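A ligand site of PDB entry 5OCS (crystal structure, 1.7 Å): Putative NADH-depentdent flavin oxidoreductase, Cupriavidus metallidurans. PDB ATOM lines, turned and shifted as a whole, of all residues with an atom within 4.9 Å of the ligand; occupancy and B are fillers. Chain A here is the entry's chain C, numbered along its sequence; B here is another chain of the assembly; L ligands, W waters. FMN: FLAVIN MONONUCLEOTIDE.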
ATOM      1  N   ALA A  22      15.630  12.323 -23.091  1.00  0.00           N
ATOM      2  CA  ALA A  22      14.301  12.483 -23.640  1.00  0.00           C
ATOM      3  C   ALA A  22      13.973  11.363 -24.631  1.00  0.00           C
ATOM      4  O   ALA A  22      14.888  10.806 -25.289  1.00  0.00           O
ATOM      5  CB  ALA A  22      14.222  13.833 -24.352  1.00  0.00           C
ATOM      6  N   PRO A  23      12.671  11.020 -24.776  1.00  0.00           N
ATOM      7  CA  PRO A  23      12.293   9.993 -25.737  1.00  0.00           C
ATOM      8  C   PRO A  23      12.710  10.389 -27.162  1.00  0.00           C
ATOM      9  O   PRO A  23      12.524  11.566 -27.592  1.00  0.00           O
ATOM     10  CB  PRO A  23      10.768   9.901 -25.589  1.00  0.00           C
ATOM     11  CG  PRO A  23      10.366  11.278 -25.119  1.00  0.00           C
ATOM     12  CD  PRO A  23      11.488  11.667 -24.163  1.00  0.00           C
ATOM     13  N   MET A  24      13.327   9.441 -27.861  1.00  0.00           N
ATOM     14  CA  MET A  24      13.817   9.712 -29.239  1.00  0.00           C
ATOM     15  C   MET A  24      13.557   8.540 -30.155  1.00  0.00           C
ATOM     16  O   MET A  24      14.287   7.568 -30.126  1.00  0.00           O
ATOM     17  CB  MET A  24      15.297  10.093 -29.309  1.00  0.00           C
ATOM     18  CG  MET A  24      15.598  11.422 -28.703  1.00  0.00           C
ATOM     19  SD  MET A  24      17.384  11.800 -28.704  1.00  0.00           S
ATOM     20  CE  MET A  24      17.925  10.796 -27.307  1.00  0.00           C
ATOM     21  N   CYS A  25      12.527   8.662 -30.974  1.00  0.00           N
ATOM     22  CA  CYS A  25      12.236   7.679 -32.031  1.00  0.00           C
ATOM     23  C   CYS A  25      13.442   7.382 -32.878  1.00  0.00           C
ATOM     24  O   CYS A  25      14.131   8.295 -33.354  1.00  0.00           O
ATOM     25  CB  CYS A  25      11.163   8.195 -32.960  1.00  0.00           C
ATOM     26  SG  CYS A  25       9.492   8.069 -32.265  1.00  0.00           S
ATOM     27  N   TYR A  27      12.966   4.828 -35.395  1.00  0.00           N
ATOM     28  CA  TYR A  27      12.379   4.320 -36.619  1.00  0.00           C
ATOM     29  C   TYR A  27      13.153   3.067 -37.132  1.00  0.00           C
ATOM     30  O   TYR A  27      13.362   2.901 -38.329  1.00  0.00           O
ATOM     31  CB  TYR A  27      12.290   5.404 -37.691  1.00  0.00           C
ATOM     32  CG  TYR A  27      11.821   6.718 -37.173  1.00  0.00           C
ATOM     33  CD1 TYR A  27      12.723   7.646 -36.691  1.00  0.00           C
ATOM     34  CD2 TYR A  27      10.472   7.041 -37.190  1.00  0.00           C
ATOM     35  CE1 TYR A  27      12.311   8.855 -36.193  1.00  0.00           C
ATOM     36  CE2 TYR A  27      10.026   8.251 -36.684  1.00  0.00           C
ATOM     37  CZ  TYR A  27      10.955   9.125 -36.156  1.00  0.00           C
ATOM     38  OH  TYR A  27      10.529  10.368 -35.698  1.00  0.00           O
ATOM     39  N   GLU A  56      11.867   5.802 -26.485  1.00  0.00           N
ATOM     40  CA  GLU A  56      11.073   6.399 -27.555  1.00  0.00           C
ATOM     41  C   GLU A  56       9.585   6.108 -27.562  1.00  0.00           C
ATOM     42  O   GLU A  56       9.169   5.055 -27.034  1.00  0.00           O
ATOM     43  CB  GLU A  56      11.623   5.939 -28.887  1.00  0.00           C
ATOM     44  CG  GLU A  56      11.502   4.458 -29.193  1.00  0.00           C
ATOM     45  CD  GLU A  56      12.315   4.049 -30.409  1.00  0.00           C
ATOM     46  OE1 GLU A  56      11.908   4.253 -31.578  1.00  0.00           O
ATOM     47  OE2 GLU A  56      13.387   3.502 -30.150  1.00  0.00           O
ATOM     48  N   ALA A  57       8.831   6.979 -28.246  1.00  0.00           N
ATOM     49  CA  ALA A  57       7.398   6.756 -28.569  1.00  0.00           C
ATOM     50  C   ALA A  57       7.191   5.313 -28.973  1.00  0.00           C
ATOM     51  O   ALA A  57       7.624   4.867 -30.006  1.00  0.00           O
ATOM     52  CB  ALA A  57       6.891   7.709 -29.620  1.00  0.00           C
ATOM     53  N   GLN A 100       7.841   5.832 -23.062  1.00  0.00           N
ATOM     54  CA  GLN A 100       6.800   6.717 -23.545  1.00  0.00           C
ATOM     55  C   GLN A 100       5.840   5.866 -24.353  1.00  0.00           C
ATOM     56  O   GLN A 100       6.217   5.259 -25.354  1.00  0.00           O
ATOM     57  CB  GLN A 100       7.388   7.852 -24.401  1.00  0.00           C
ATOM     58  CG  GLN A 100       6.341   8.870 -24.823  1.00  0.00           C
ATOM     59  CD  GLN A 100       6.864   9.892 -25.773  1.00  0.00           C
ATOM     60  OE1 GLN A 100       7.213   9.558 -26.928  1.00  0.00           O
ATOM     61  NE2 GLN A 100       6.889  11.134 -25.336  1.00  0.00           N
ATOM     62  N   GLU A 176       5.584   7.394 -19.347  1.00  0.00           N
ATOM     63  CA  GLU A 176       5.276   8.735 -19.840  1.00  0.00           C
ATOM     64  C   GLU A 176       4.202   8.554 -20.926  1.00  0.00           C
ATOM     65  O   GLU A 176       4.418   7.922 -21.952  1.00  0.00           O
ATOM     66  CB  GLU A 176       6.511   9.412 -20.441  1.00  0.00           C
ATOM     67  CG  GLU A 176       6.175  10.764 -21.060  1.00  0.00           C
ATOM     68  CD  GLU A 176       7.419  11.505 -21.441  1.00  0.00           C
ATOM     69  OE1 GLU A 176       8.079  12.094 -20.540  1.00  0.00           O
ATOM     70  OE2 GLU A 176       7.737  11.472 -22.646  1.00  0.00           O
ATOM     71  N   HIS A 178       2.220   9.871 -23.902  1.00  0.00           N
ATOM     72  CA  HIS A 178       2.554  10.897 -24.900  1.00  0.00           C
ATOM     73  C   HIS A 178       1.311  11.715 -25.195  1.00  0.00           C
ATOM     74  O   HIS A 178       0.405  11.260 -25.885  1.00  0.00           O
ATOM     75  CB  HIS A 178       3.092  10.232 -26.177  1.00  0.00           C
ATOM     76  CG  HIS A 178       3.873  11.152 -27.069  1.00  0.00           C
ATOM     77  ND1 HIS A 178       3.807  12.508 -26.978  1.00  0.00           N
ATOM     78  CD2 HIS A 178       4.722  10.881 -28.088  1.00  0.00           C
ATOM     79  CE1 HIS A 178       4.593  13.061 -27.880  1.00  0.00           C
ATOM     80  NE2 HIS A 178       5.185  12.089 -28.558  1.00  0.00           N
ATOM     81  N   HIS A 181       3.164  16.881 -29.264  1.00  0.00           N
ATOM     82  CA  HIS A 181       3.715  16.762 -30.633  1.00  0.00           C
ATOM     83  C   HIS A 181       2.728  16.456 -31.736  1.00  0.00           C
ATOM     84  O   HIS A 181       3.051  15.854 -32.739  1.00  0.00           O
ATOM     85  CB  HIS A 181       4.941  15.838 -30.644  1.00  0.00           C
ATOM     86  CG  HIS A 181       6.023  16.314 -29.745  1.00  0.00           C
ATOM     87  ND1 HIS A 181       7.127  15.559 -29.418  1.00  0.00           N
ATOM     88  CD2 HIS A 181       6.190  17.513 -29.118  1.00  0.00           C
ATOM     89  CE1 HIS A 181       7.911  16.252 -28.610  1.00  0.00           C
ATOM     90  NE2 HIS A 181       7.361  17.453 -28.415  1.00  0.00           N
ATOM     91  N   ARG A 231       3.676  13.748 -21.105  1.00  0.00           N
ATOM     92  CA  ARG A 231       4.388  14.771 -21.840  1.00  0.00           C
ATOM     93  C   ARG A 231       3.313  15.591 -22.576  1.00  0.00           C
ATOM     94  O   ARG A 231       2.426  15.030 -23.225  1.00  0.00           O
ATOM     95  CB  ARG A 231       5.372  14.143 -22.818  1.00  0.00           C
ATOM     96  CG  ARG A 231       6.328  15.157 -23.412  1.00  0.00           C
ATOM     97  CD  ARG A 231       7.485  14.567 -24.228  1.00  0.00           C
ATOM     98  NE  ARG A 231       8.724  15.369 -24.080  1.00  0.00           N
ATOM     99  CZ  ARG A 231       9.758  15.384 -24.942  1.00  0.00           C
ATOM    100  NH1 ARG A 231       9.705  14.722 -26.085  1.00  0.00           N
ATOM    101  NH2 ARG A 231      10.865  16.108 -24.683  1.00  0.00           N
ATOM    102  N   SER A 265       7.012  20.067 -23.458  1.00  0.00           N
ATOM    103  CA  SER A 265       7.523  20.385 -24.798  1.00  0.00           C
ATOM    104  C   SER A 265       6.512  21.387 -25.457  1.00  0.00           C
ATOM    105  O   SER A 265       5.707  22.049 -24.770  1.00  0.00           O
ATOM    106  CB  SER A 265       7.655  19.074 -25.611  1.00  0.00           C
ATOM    107  OG  SER A 265       8.199  19.368 -26.905  1.00  0.00           O
ATOM    108  N   VAL A 300      12.729  20.850 -21.626  1.00  0.00           N
ATOM    109  CA  VAL A 300      13.461  20.362 -22.772  1.00  0.00           C
ATOM    110  C   VAL A 300      13.542  21.441 -23.852  1.00  0.00           C
ATOM    111  O   VAL A 300      12.638  22.315 -23.902  1.00  0.00           O
ATOM    112  CB  VAL A 300      12.771  19.094 -23.323  1.00  0.00           C
ATOM    113  CG1 VAL A 300      11.419  19.391 -23.963  1.00  0.00           C
ATOM    114  CG2 VAL A 300      13.655  18.308 -24.280  1.00  0.00           C
ATOM    115  N   GLY A 301      14.546  21.356 -24.730  1.00  0.00           N
ATOM    116  CA  GLY A 301      14.583  22.111 -25.992  1.00  0.00           C
ATOM    117  C   GLY A 301      15.835  22.956 -26.164  1.00  0.00           C
ATOM    118  O   GLY A 301      15.939  24.038 -25.618  1.00  0.00           O
ATOM    119  N   LEU A 302      16.812  22.419 -26.867  1.00  0.00           N
ATOM    120  CA  LEU A 302      18.053  23.127 -27.174  1.00  0.00           C
ATOM    121  C   LEU A 302      18.775  23.480 -25.858  1.00  0.00           C
ATOM    122  O   LEU A 302      19.309  24.564 -25.696  1.00  0.00           O
ATOM    123  CB  LEU A 302      17.796  24.354 -28.094  1.00  0.00           C
ATOM    124  CG  LEU A 302      17.391  24.010 -29.528  1.00  0.00           C
ATOM    125  CD1 LEU A 302      16.909  25.242 -30.285  1.00  0.00           C
ATOM    126  CD2 LEU A 302      18.561  23.427 -30.344  1.00  0.00           C
ATOM    127  N   ILE A 303      18.760  22.513 -24.948  1.00  0.00           N
ATOM    128  CA  ILE A 303      19.597  22.529 -23.761  1.00  0.00           C
ATOM    129  C   ILE A 303      20.775  21.638 -24.098  1.00  0.00           C
ATOM    130  O   ILE A 303      20.602  20.421 -24.218  1.00  0.00           O
ATOM    131  CB  ILE A 303      18.840  22.040 -22.524  1.00  0.00           C
ATOM    132  CG1 ILE A 303      17.629  22.964 -22.314  1.00  0.00           C
ATOM    133  CG2 ILE A 303      19.753  22.071 -21.290  1.00  0.00           C
ATOM    134  CD1 ILE A 303      16.606  22.432 -21.333  1.00  0.00           C
ATOM    135  N   SER A 322      15.601  17.561 -19.509  1.00  0.00           N
ATOM    136  CA  SER A 322      15.518  16.528 -20.557  1.00  0.00           C
ATOM    137  C   SER A 322      16.387  16.948 -21.733  1.00  0.00           C
ATOM    138  O   SER A 322      16.334  18.126 -22.147  1.00  0.00           O
ATOM    139  CB  SER A 322      14.082  16.381 -21.037  1.00  0.00           C
ATOM    140  OG  SER A 322      13.255  15.805 -20.050  1.00  0.00           O
ATOM    141  N   ILE A 323      17.185  16.027 -22.260  1.00  0.00           N
ATOM    142  CA  ILE A 323      18.096  16.292 -23.362  1.00  0.00           C
ATOM    143  C   ILE A 323      17.897  15.203 -24.416  1.00  0.00           C
ATOM    144  O   ILE A 323      17.865  14.022 -24.090  1.00  0.00           O
ATOM    145  CB  ILE A 323      19.507  16.240 -22.859  1.00  0.00           C
ATOM    146  CG1 ILE A 323      19.739  17.305 -21.788  1.00  0.00           C
ATOM    147  CG2 ILE A 323      20.498  16.469 -23.996  1.00  0.00           C
ATOM    148  CD1 ILE A 323      20.978  17.050 -20.969  1.00  0.00           C
ATOM    149  N   ALA A 324      17.780  15.607 -25.665  1.00  0.00           N
ATOM    150  CA  ALA A 324      17.665  14.672 -26.783  1.00  0.00           C
ATOM    151  C   ALA A 324      18.850  14.788 -27.723  1.00  0.00           C
ATOM    152  O   ALA A 324      19.803  14.036 -27.656  1.00  0.00           O
ATOM    153  CB  ALA A 324      16.335  14.891 -27.503  1.00  0.00           C
ATOM    154  N   ARG A 325      18.839  15.772 -28.593  1.00  0.00           N
ATOM    155  CA  ARG A 325      19.893  15.842 -29.587  1.00  0.00           C
ATOM    156  C   ARG A 325      21.304  15.914 -28.995  1.00  0.00           C
ATOM    157  O   ARG A 325      22.221  15.293 -29.558  1.00  0.00           O
ATOM    158  CB  ARG A 325      19.677  17.014 -30.524  1.00  0.00           C
ATOM    159  CG  ARG A 325      18.547  16.743 -31.504  1.00  0.00           C
ATOM    160  CD  ARG A 325      18.123  17.989 -32.269  1.00  0.00           C
ATOM    161  NE  ARG A 325      17.414  18.906 -31.394  1.00  0.00           N
ATOM    162  CZ  ARG A 325      16.803  20.016 -31.784  1.00  0.00           C
ATOM    163  NH1 ARG A 325      16.824  20.357 -33.065  1.00  0.00           N
ATOM    164  NH2 ARG A 325      16.148  20.780 -30.912  1.00  0.00           N
ATOM    165  N   ALA A 326      21.510  16.687 -27.921  1.00  0.00           N
ATOM    166  CA  ALA A 326      22.845  16.722 -27.294  1.00  0.00           C
ATOM    167  C   ALA A 326      23.314  15.352 -26.791  1.00  0.00           C
ATOM    168  O   ALA A 326      24.538  15.109 -26.762  1.00  0.00           O
ATOM    169  CB  ALA A 326      22.947  17.755 -26.220  1.00  0.00           C
ATOM    170  N   LEU A 328      22.483  12.425 -28.409  1.00  0.00           N
ATOM    171  CA  LEU A 328      22.878  11.738 -29.639  1.00  0.00           C
ATOM    172  C   LEU A 328      24.244  12.228 -30.074  1.00  0.00           C
ATOM    173  O   LEU A 328      25.062  11.441 -30.476  1.00  0.00           O
ATOM    174  CB  LEU A 328      21.836  11.957 -30.736  1.00  0.00           C
ATOM    175  CG  LEU A 328      20.422  11.511 -30.413  1.00  0.00           C
ATOM    176  CD1 LEU A 328      19.560  11.677 -31.654  1.00  0.00           C
ATOM    177  CD2 LEU A 328      20.412  10.078 -29.902  1.00  0.00           C
ATOM    178  N   GLN B 350      19.748   7.381 -38.221  1.00  0.00           N
ATOM    179  CA  GLN B 350      18.969   7.550 -36.977  1.00  0.00           C
ATOM    180  C   GLN B 350      19.425   8.752 -36.139  1.00  0.00           C
ATOM    181  O   GLN B 350      18.678   9.263 -35.276  1.00  0.00           O
ATOM    182  CB  GLN B 350      19.045   6.320 -36.079  1.00  0.00           C
ATOM    183  CG  GLN B 350      18.414   5.040 -36.601  1.00  0.00           C
ATOM    184  CD  GLN B 350      19.304   4.204 -37.551  1.00  0.00           C
ATOM    185  OE1 GLN B 350      20.344   4.664 -38.068  1.00  0.00           O
ATOM    186  NE2 GLN B 350      18.827   3.008 -37.871  1.00  0.00           N
ATOM    187  N   ARG B 353      19.690  14.044 -37.113  1.00  0.00           N
ATOM    188  CA  ARG B 353      19.112  15.245 -36.484  1.00  0.00           C
ATOM    189  C   ARG B 353      19.913  15.768 -35.309  1.00  0.00           C
ATOM    190  O   ARG B 353      19.609  16.847 -34.818  1.00  0.00           O
ATOM    191  CB  ARG B 353      17.658  14.987 -36.046  1.00  0.00           C
ATOM    192  CG  ARG B 353      16.751  14.723 -37.221  1.00  0.00           C
ATOM    193  CD  ARG B 353      15.555  13.865 -36.876  1.00  0.00           C
ATOM    194  NE  ARG B 353      14.603  14.491 -35.966  1.00  0.00           N
ATOM    195  CZ  ARG B 353      13.511  13.899 -35.506  1.00  0.00           C
ATOM    196  NH1 ARG B 353      13.211  12.645 -35.873  1.00  0.00           N
ATOM    197  NH2 ARG B 353      12.700  14.551 -34.656  1.00  0.00           N
HETATM  198  N1  FMN L   1       9.697  13.457 -28.576  1.00  0.00           N
HETATM  199  C2  FMN L   1       8.795  12.524 -28.098  1.00  0.00           C
HETATM  200  O2  FMN L   1       7.952  12.961 -27.258  1.00  0.00           O
HETATM  201  N3  FMN L   1       8.800  11.226 -28.445  1.00  0.00           N
HETATM  202  C4  FMN L   1       9.687  10.731 -29.288  1.00  0.00           C
HETATM  203  O4  FMN L   1       9.733   9.544 -29.544  1.00  0.00           O
HETATM  204  C4A FMN L   1      10.640  11.643 -29.911  1.00  0.00           C
HETATM  205  N5  FMN L   1      11.503  11.183 -30.845  1.00  0.00           N
HETATM  206  C5A FMN L   1      12.535  12.005 -31.285  1.00  0.00           C
HETATM  207  C6  FMN L   1      13.519  11.502 -32.144  1.00  0.00           C
HETATM  208  C7  FMN L   1      14.541  12.312 -32.601  1.00  0.00           C
HETATM  209  C7M FMN L   1      15.571  11.759 -33.544  1.00  0.00           C
HETATM  210  C8  FMN L   1      14.561  13.709 -32.156  1.00  0.00           C
HETATM  211  C8M FMN L   1      15.625  14.677 -32.628  1.00  0.00           C
HETATM  212  C9  FMN L   1      13.608  14.216 -31.287  1.00  0.00           C
HETATM  213  C9A FMN L   1      12.587  13.420 -30.804  1.00  0.00           C
HETATM  214  N10 FMN L   1      11.600  13.927 -29.928  1.00  0.00           N
HETATM  215  C10 FMN L   1      10.634  13.016 -29.445  1.00  0.00           C
HETATM  216  C1' FMN L   1      11.645  15.262 -29.415  1.00  0.00           C
HETATM  217  C2' FMN L   1      12.729  15.201 -28.304  1.00  0.00           C
HETATM  218  O2' FMN L   1      12.323  14.360 -27.199  1.00  0.00           O
HETATM  219  C3' FMN L   1      13.011  16.612 -27.745  1.00  0.00           C
HETATM  220  O3' FMN L   1      11.816  17.081 -27.084  1.00  0.00           O
HETATM  221  C4' FMN L   1      13.431  17.604 -28.833  1.00  0.00           C
HETATM  222  O4' FMN L   1      14.400  17.032 -29.701  1.00  0.00           O
HETATM  223  C5' FMN L   1      13.977  18.877 -28.212  1.00  0.00           C
HETATM  224  O5' FMN L   1      15.065  18.627 -27.329  1.00  0.00           O
HETATM  225  P   FMN L   1      16.597  18.720 -27.794  1.00  0.00           P
HETATM  226  O1P FMN L   1      16.807  17.758 -28.967  1.00  0.00           O
HETATM  227  O2P FMN L   1      16.704  20.163 -28.188  1.00  0.00           O
HETATM  228  O3P FMN L   1      17.286  18.379 -26.507  1.00  0.00           O
HETATM  229  O   HOH W   1      13.953  17.865 -32.303  1.00  0.00           O
HETATM  230  O   HOH W   2      11.546  16.466 -32.953  1.00  0.00           O
HETATM  231  O   HOH W   3      10.794  19.407 -27.612  1.00  0.00           O
HETATM  232  O   HOH W   4      10.395  13.525 -33.552  1.00  0.00           O
HETATM  233  O   HOH W   5      19.589  20.440 -28.739  1.00  0.00           O
HETATM  234  O   HOH W   6      19.958  18.771 -26.460  1.00  0.00           O
HETATM  235  O   HOH W   7      16.926  19.892 -24.376  1.00  0.00           O
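N of Leu 302 lies within hydrogen-bond range of O2P of the ligand (2.6 Å). A nitrogen (N5) of the ligand sits at hydrogen-bond distance from the backbone NH of Cys 25, at 2.7 Å. O4 of the ligand lies within hydrogen-bond range of SG of Cys 25, at 3.1 Å. O2 of the ligand is in hydrogen-bond range of NH1 of Arg 231. N of Arg 325 lies within hydrogen-bond range of O1P of the ligand (2.9 Å). An oxygen (O1P) of the ligand lies within salt-bridge range of the guanidinium group (NE) of Arg 325 (2.8 Å). N3 of the ligand lies within hydrogen-bond range of OE1 of Gln 100, 2.8 Å away. O2' of the ligand is in hydrogen-bond range of O of Pro 23 (2.8 Å). O3P of the ligand lies within hydrogen-bond range of N of Ala 324, 2.9 Å away. N of Ala 57 lies within hydrogen-bond range of O4 of the ligand (3.0 Å). An oxygen (O2) of the ligand is in hydrogen-bond range of a ring nitrogen (NE2) of His 178 (3.2 Å). A nitrogen (N1) of the ligand sits close to a ring nitrogen (ND1) of His 181 (3.4 Å).
OE1 of Gln 100 sits close to N of Ala 57, at 3.3 Å. The side-chain amide nitrogen (NE2) of Gln 100 lies within hydrogen-bond range of the side-chain carboxylate (OE2) of Glu 176, 2.8 Å away. The side-chain hydroxyl (OG) of Ser 265 sits at hydrogen-bond distance from a ring nitrogen (NE2) of His 181 (2.6 Å). The backbone carbonyl oxygen (O) of Ile 323 is in hydrogen-bond range of the backbone NH (N) of Ala 22.
Merely in contact with the ligand: Ala 22 (3.5 Å), Met 24 (3.2 Å), Glu 56 (3.96 Å), Val 300 (3.4 Å), Gly 301 (3.6 Å), Ile 323 (3.9 Å) and Arg 353 of chain B (3.2 Å). Within 4 Å of the ligand: Ala 22, Pro 23, Met 24, Cys 25, Glu 56, Ala 57, Gln 100, His 178, His 181, Arg 231, Val 300, Gly 301, Leu 302, Ile 323, Ala 324, Arg 325 and Arg 353 of chain B.
Water W3 lies within hydrogen-bond range of an oxygen (O3') of the ligand (2.6 Å) and the side-chain hydroxyl (OG) of Ser 265 (2.7 Å). Water W7 lies within hydrogen-bond range of O3P of the ligand (2.6 Å), N of Gly 301 (2.8 Å), O of Ser 322 (2.9 Å) and N of Ile 303 (3.2 Å). Water W6 lies within hydrogen-bond range of an oxygen (O3P) of the ligand, the backbone carbonyl oxygen of Ile 303 and the backbone NH of Ala 326.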
